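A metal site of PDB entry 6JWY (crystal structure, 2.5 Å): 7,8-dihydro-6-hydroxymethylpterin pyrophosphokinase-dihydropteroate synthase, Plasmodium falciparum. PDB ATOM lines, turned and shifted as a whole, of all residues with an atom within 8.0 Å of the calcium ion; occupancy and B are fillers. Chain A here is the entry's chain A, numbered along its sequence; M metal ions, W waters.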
ATOM      1  N   LEU A  38       8.850  15.569  -3.817  1.00  0.00           N
ATOM      2  CA  LEU A  38       9.167  15.448  -2.398  1.00  0.00           C
ATOM      3  C   LEU A  38       8.430  16.557  -1.662  1.00  0.00           C
ATOM      4  O   LEU A  38       7.824  16.284  -0.629  1.00  0.00           O
ATOM      5  CB  LEU A  38      10.677  15.509  -2.123  1.00  0.00           C
ATOM      6  CG  LEU A  38      11.517  14.285  -2.525  1.00  0.00           C
ATOM      7  CD1 LEU A  38      12.966  14.499  -2.131  1.00  0.00           C
ATOM      8  CD2 LEU A  38      10.993  13.003  -1.872  1.00  0.00           C
ATOM      9  N   HIS A  39       8.458  17.780  -2.214  1.00  0.00           N
ATOM     10  CA  HIS A  39       7.818  18.909  -1.569  1.00  0.00           C
ATOM     11  C   HIS A  39       6.333  18.645  -1.384  1.00  0.00           C
ATOM     12  O   HIS A  39       5.792  18.888  -0.313  1.00  0.00           O
ATOM     13  CB  HIS A  39       8.069  20.257  -2.283  1.00  0.00           C
ATOM     14  CG  HIS A  39       9.474  20.772  -2.192  1.00  0.00           C
ATOM     15  ND1 HIS A  39      10.233  21.060  -3.319  1.00  0.00           N
ATOM     16  CD2 HIS A  39      10.256  21.086  -1.127  1.00  0.00           C
ATOM     17  CE1 HIS A  39      11.418  21.514  -2.955  1.00  0.00           C
ATOM     18  NE2 HIS A  39      11.457  21.541  -1.601  1.00  0.00           N
ATOM     19  N   LEU A  40       5.684  18.102  -2.432  1.00  0.00           N
ATOM     20  CA  LEU A  40       4.255  17.869  -2.368  1.00  0.00           C
ATOM     21  C   LEU A  40       3.927  16.710  -1.430  1.00  0.00           C
ATOM     22  O   LEU A  40       2.931  16.771  -0.725  1.00  0.00           O
ATOM     23  CB  LEU A  40       3.717  17.672  -3.790  1.00  0.00           C
ATOM     24  CG  LEU A  40       3.985  18.880  -4.689  1.00  0.00           C
ATOM     25  CD1 LEU A  40       3.543  18.646  -6.120  1.00  0.00           C
ATOM     26  CD2 LEU A  40       3.356  20.142  -4.119  1.00  0.00           C
ATOM     27  N   VAL A  41       4.796  15.703  -1.371  1.00  0.00           N
ATOM     28  CA  VAL A  41       4.671  14.663  -0.361  1.00  0.00           C
ATOM     29  C   VAL A  41       4.741  15.291   1.040  1.00  0.00           C
ATOM     30  O   VAL A  41       3.946  14.935   1.900  1.00  0.00           O
ATOM     31  CB  VAL A  41       5.747  13.575  -0.528  1.00  0.00           C
ATOM     32  CG1 VAL A  41       5.680  12.535   0.580  1.00  0.00           C
ATOM     33  CG2 VAL A  41       5.676  12.922  -1.896  1.00  0.00           C
ATOM     34  N   GLU A  42       5.682  16.219   1.256  1.00  0.00           N
ATOM     35  CA  GLU A  42       5.843  16.846   2.562  1.00  0.00           C
ATOM     36  C   GLU A  42       4.612  17.684   2.878  1.00  0.00           C
ATOM     37  O   GLU A  42       4.245  17.860   4.046  1.00  0.00           O
ATOM     38  CB  GLU A  42       6.967  17.879   2.565  1.00  0.00           C
ATOM     39  CG  GLU A  42       8.222  17.489   3.327  1.00  0.00           C
ATOM     40  CD  GLU A  42       8.197  17.137   4.812  1.00  0.00           C
ATOM     41  OE1 GLU A  42       7.242  17.561   5.544  1.00  0.00           O
ATOM     42  OE2 GLU A  42       9.158  16.424   5.229  1.00  0.00           O
ATOM     43  N   LYS A  43       4.023  18.261   1.822  1.00  0.00           N
ATOM     44  CA  LYS A  43       2.950  19.222   1.989  1.00  0.00           C
ATOM     45  C   LYS A  43       1.639  18.487   2.251  1.00  0.00           C
ATOM     46  O   LYS A  43       0.922  18.890   3.150  1.00  0.00           O
ATOM     47  CB  LYS A  43       2.856  20.177   0.796  1.00  0.00           C
ATOM     48  CG  LYS A  43       1.812  21.274   0.925  1.00  0.00           C
ATOM     49  CD  LYS A  43       1.711  22.063  -0.347  1.00  0.00           C
ATOM     50  CE  LYS A  43       0.893  23.318  -0.166  1.00  0.00           C
ATOM     51  NZ  LYS A  43       1.610  24.330   0.633  1.00  0.00           N
ATOM     52  N   TYR A  44       1.367  17.415   1.498  1.00  0.00           N
ATOM     53  CA  TYR A  44       0.050  16.780   1.454  1.00  0.00           C
ATOM     54  C   TYR A  44       0.004  15.420   2.139  1.00  0.00           C
ATOM     55  O   TYR A  44      -1.079  14.938   2.469  1.00  0.00           O
ATOM     56  CB  TYR A  44      -0.463  16.669   0.014  1.00  0.00           C
ATOM     57  CG  TYR A  44      -0.738  17.983  -0.687  1.00  0.00           C
ATOM     58  CD1 TYR A  44      -1.487  18.982  -0.078  1.00  0.00           C
ATOM     59  CD2 TYR A  44      -0.264  18.215  -1.962  1.00  0.00           C
ATOM     60  CE1 TYR A  44      -1.734  20.184  -0.723  1.00  0.00           C
ATOM     61  CE2 TYR A  44      -0.505  19.410  -2.625  1.00  0.00           C
ATOM     62  CZ  TYR A  44      -1.243  20.398  -1.996  1.00  0.00           C
ATOM     63  OH  TYR A  44      -1.488  21.576  -2.641  1.00  0.00           O
ATOM     64  N   LEU A  45       1.151  14.764   2.377  1.00  0.00           N
ATOM     65  CA  LEU A  45       1.062  13.387   2.850  1.00  0.00           C
ATOM     66  C   LEU A  45       1.507  13.201   4.293  1.00  0.00           C
ATOM     67  O   LEU A  45       1.024  12.276   4.943  1.00  0.00           O
ATOM     68  CB  LEU A  45       1.775  12.451   1.872  1.00  0.00           C
ATOM     69  CG  LEU A  45       1.123  12.420   0.489  1.00  0.00           C
ATOM     70  CD1 LEU A  45       1.873  11.497  -0.459  1.00  0.00           C
ATOM     71  CD2 LEU A  45      -0.328  11.991   0.631  1.00  0.00           C
ATOM     72  N   GLY A  46       2.420  14.040   4.799  1.00  0.00           N
ATOM     73  CA  GLY A  46       2.964  13.871   6.142  1.00  0.00           C
ATOM     74  C   GLY A  46       4.410  14.346   6.240  1.00  0.00           C
ATOM     75  O   GLY A  46       4.757  15.386   5.690  1.00  0.00           O
ATOM     76  N   LYS A  47       5.245  13.569   6.951  1.00  0.00           N
ATOM     77  CA  LYS A  47       6.630  13.910   7.202  1.00  0.00           C
ATOM     78  C   LYS A  47       7.540  12.911   6.497  1.00  0.00           C
ATOM     79  O   LYS A  47       7.411  11.697   6.706  1.00  0.00           O
ATOM     80  CB  LYS A  47       6.981  13.897   8.698  1.00  0.00           C
ATOM     81  CG  LYS A  47       8.326  14.554   8.993  1.00  0.00           C
ATOM     82  CD  LYS A  47       8.751  14.666  10.448  1.00  0.00           C
ATOM     83  CE  LYS A  47      10.080  15.369  10.637  1.00  0.00           C
ATOM     84  NZ  LYS A  47      10.170  16.632   9.838  1.00  0.00           N
ATOM     85  N   ILE A  48       8.460  13.425   5.679  1.00  0.00           N
ATOM     86  CA  ILE A  48       9.464  12.576   5.055  1.00  0.00           C
ATOM     87  C   ILE A  48      10.516  12.221   6.098  1.00  0.00           C
ATOM     88  O   ILE A  48      11.166  13.112   6.633  1.00  0.00           O
ATOM     89  CB  ILE A  48      10.075  13.268   3.820  1.00  0.00           C
ATOM     90  CG1 ILE A  48       9.023  13.448   2.726  1.00  0.00           C
ATOM     91  CG2 ILE A  48      11.283  12.487   3.301  1.00  0.00           C
ATOM     92  CD1 ILE A  48       9.559  13.998   1.426  1.00  0.00           C
ATOM     93  N   SER A  95      -2.655  22.637   2.706  1.00  0.00           N
ATOM     94  CA  SER A  95      -2.955  21.377   3.366  1.00  0.00           C
ATOM     95  C   SER A  95      -3.728  21.694   4.637  1.00  0.00           C
ATOM     96  O   SER A  95      -3.546  22.752   5.230  1.00  0.00           O
ATOM     97  CB  SER A  95      -1.696  20.581   3.656  1.00  0.00           C
ATOM     98  OG  SER A  95      -1.839  19.733   4.793  1.00  0.00           O
ATOM     99  N   TYR A  97      -3.329  19.976   7.134  1.00  0.00           N
ATOM    100  CA  TYR A  97      -2.486  19.454   8.204  1.00  0.00           C
ATOM    101  C   TYR A  97      -1.246  20.322   8.384  1.00  0.00           C
ATOM    102  O   TYR A  97      -0.712  20.837   7.405  1.00  0.00           O
ATOM    103  CB  TYR A  97      -2.122  18.002   7.937  1.00  0.00           C
ATOM    104  CG  TYR A  97      -3.249  17.049   8.217  1.00  0.00           C
ATOM    105  CD1 TYR A  97      -4.283  16.895   7.308  1.00  0.00           C
ATOM    106  CD2 TYR A  97      -3.315  16.339   9.411  1.00  0.00           C
ATOM    107  CE1 TYR A  97      -5.345  16.050   7.551  1.00  0.00           C
ATOM    108  CE2 TYR A  97      -4.368  15.470   9.668  1.00  0.00           C
ATOM    109  CZ  TYR A  97      -5.387  15.327   8.736  1.00  0.00           C
ATOM    110  OH  TYR A  97      -6.419  14.473   8.959  1.00  0.00           O
ATOM    111  N   GLU A  98      -0.796  20.469   9.639  1.00  0.00           N
ATOM    112  CA  GLU A  98       0.261  21.437   9.910  1.00  0.00           C
ATOM    113  C   GLU A  98       1.593  20.839   9.478  1.00  0.00           C
ATOM    114  O   GLU A  98       1.860  19.670   9.740  1.00  0.00           O
ATOM    115  CB  GLU A  98       0.415  21.843  11.389  1.00  0.00           C
ATOM    116  CG  GLU A  98      -0.708  21.459  12.335  1.00  0.00           C
ATOM    117  CD  GLU A  98      -0.531  20.090  12.960  1.00  0.00           C
ATOM    118  OE1 GLU A  98       0.525  19.870  13.628  1.00  0.00           O
ATOM    119  OE2 GLU A  98      -1.440  19.238  12.779  1.00  0.00           O
ATOM    120  N   GLU A  99       2.425  21.672   8.880  1.00  0.00           N
ATOM    121  CA  GLU A  99       3.847  21.405   8.768  1.00  0.00           C
ATOM    122  C   GLU A  99       4.519  21.690  10.116  1.00  0.00           C
ATOM    123  O   GLU A  99       4.186  22.671  10.789  1.00  0.00           O
ATOM    124  CB  GLU A  99       4.439  22.285   7.684  1.00  0.00           C
ATOM    125  CG  GLU A  99       5.778  21.799   7.173  1.00  0.00           C
ATOM    126  CD  GLU A  99       5.746  20.390   6.598  1.00  0.00           C
ATOM    127  OE1 GLU A  99       5.446  20.243   5.392  1.00  0.00           O
ATOM    128  OE2 GLU A  99       5.975  19.462   7.380  1.00  0.00           O
ATOM    129  N   ASN A 100       5.425  20.810  10.531  1.00  0.00           N
ATOM    130  CA  ASN A 100       6.241  20.981  11.714  1.00  0.00           C
ATOM    131  C   ASN A 100       7.698  20.783  11.333  1.00  0.00           C
ATOM    132  O   ASN A 100       8.138  19.658  11.064  1.00  0.00           O
ATOM    133  CB  ASN A 100       5.776  20.081  12.859  1.00  0.00           C
ATOM    134  CG  ASN A 100       4.356  20.371  13.303  1.00  0.00           C
ATOM    135  OD1 ASN A 100       3.941  21.519  13.412  1.00  0.00           O
ATOM    136  ND2 ASN A 100       3.586  19.326  13.570  1.00  0.00           N
ATOM    137  N   LYS A 101       8.469  21.879  11.295  1.00  0.00           N
ATOM    138  CA  LYS A 101       9.867  21.764  10.950  1.00  0.00           C
ATOM    139  C   LYS A 101      10.724  21.426  12.173  1.00  0.00           C
ATOM    140  O   LYS A 101      11.906  21.201  12.009  1.00  0.00           O
ATOM    141  CB  LYS A 101      10.386  23.007  10.232  1.00  0.00           C
ATOM    142  CG  LYS A 101       9.729  23.335   8.897  1.00  0.00           C
ATOM    143  CD  LYS A 101      10.503  24.381   8.109  1.00  0.00           C
ATOM    144  CE  LYS A 101      11.722  23.799   7.417  1.00  0.00           C
ATOM    145  NZ  LYS A 101      12.636  24.833   6.862  1.00  0.00           N
ATOM    146  N   VAL A 170       7.388   8.020   4.416  1.00  0.00           N
ATOM    147  CA  VAL A 170       6.553   9.081   4.936  1.00  0.00           C
ATOM    148  C   VAL A 170       5.919   8.589   6.237  1.00  0.00           C
ATOM    149  O   VAL A 170       5.378   7.486   6.273  1.00  0.00           O
ATOM    150  CB  VAL A 170       5.478   9.511   3.921  1.00  0.00           C
ATOM    151  CG1 VAL A 170       4.892  10.876   4.278  1.00  0.00           C
ATOM    152  CG2 VAL A 170       6.053   9.546   2.514  1.00  0.00           C
ATOM    153  N   LYS A 171       6.033   9.402   7.311  1.00  0.00           N
ATOM    154  CA  LYS A 171       5.140   9.318   8.453  1.00  0.00           C
ATOM    155  C   LYS A 171       3.907  10.143   8.103  1.00  0.00           C
ATOM    156  O   LYS A 171       4.002  11.362   8.018  1.00  0.00           O
ATOM    157  CB  LYS A 171       5.803   9.869   9.718  1.00  0.00           C
ATOM    158  CG  LYS A 171       5.129   9.527  11.043  1.00  0.00           C
ATOM    159  CD  LYS A 171       5.413  10.529  12.138  1.00  0.00           C
ATOM    160  CE  LYS A 171       6.544  10.139  13.063  1.00  0.00           C
ATOM    161  NZ  LYS A 171       7.257  11.314  13.620  1.00  0.00           N
ATOM    162  N   PHE A 173      -0.394  11.132   7.825  1.00  0.00           N
ATOM    163  CA  PHE A 173      -1.630  11.312   8.559  1.00  0.00           C
ATOM    164  C   PHE A 173      -2.816  10.941   7.671  1.00  0.00           C
ATOM    165  O   PHE A 173      -3.962  11.189   8.018  1.00  0.00           O
ATOM    166  CB  PHE A 173      -1.817  12.781   8.979  1.00  0.00           C
ATOM    167  CG  PHE A 173      -1.448  13.754   7.896  1.00  0.00           C
ATOM    168  CD1 PHE A 173      -2.204  13.855   6.729  1.00  0.00           C
ATOM    169  CD2 PHE A 173      -0.324  14.562   8.030  1.00  0.00           C
ATOM    170  CE1 PHE A 173      -1.832  14.747   5.728  1.00  0.00           C
ATOM    171  CE2 PHE A 173       0.038  15.444   7.018  1.00  0.00           C
ATOM    172  CZ  PHE A 173      -0.711  15.546   5.864  1.00  0.00           C
ATOM    173  N   LYS A 518      16.047  23.060   3.991  1.00  0.00           N
ATOM    174  CA  LYS A 518      14.786  22.821   3.328  1.00  0.00           C
ATOM    175  C   LYS A 518      14.076  24.157   3.122  1.00  0.00           C
ATOM    176  O   LYS A 518      13.931  24.927   4.051  1.00  0.00           O
ATOM    177  CB  LYS A 518      13.893  21.886   4.154  1.00  0.00           C
ATOM    178  CG  LYS A 518      14.419  20.497   4.516  1.00  0.00           C
ATOM    179  CD  LYS A 518      13.885  19.981   5.860  1.00  0.00           C
ATOM    180  CE  LYS A 518      12.518  19.327   5.785  1.00  0.00           C
ATOM    181  NZ  LYS A 518      11.716  19.511   7.023  1.00  0.00           N
HETATM  182 CA    CA M   1       4.919  17.839   6.346  1.00  0.00          CA
HETATM  183  O   HOH W   1       5.065  16.403   8.650  1.00  0.00           O
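OE2 of Glu 99 binds the calcium ion (2.2 Å). The calcium ion is bound by O of Glu 42. The side-chain carboxylate (OE1) of Glu 42 is bound to the calcium ion. O of Gly 46 is bound to the calcium ion. OE1 of Glu 99 is bound to the calcium ion (2.6 Å). Water W1 binds the calcium ion, at 2.7 Å.
Of the 21 residues printed, 3 come within 4 Å of the calcium ion. The nearest printed residue that does not touch the calcium ion is Lys 47 (4.3 Å).
The side-chain carboxylate (OE2) of Glu 42 sits at hydrogen-bond distance from the backbone NH (N) of Ile 48 (3.1 Å). N of Gly 46 lies within hydrogen-bond range of O of Val 41, 3.4 Å away.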
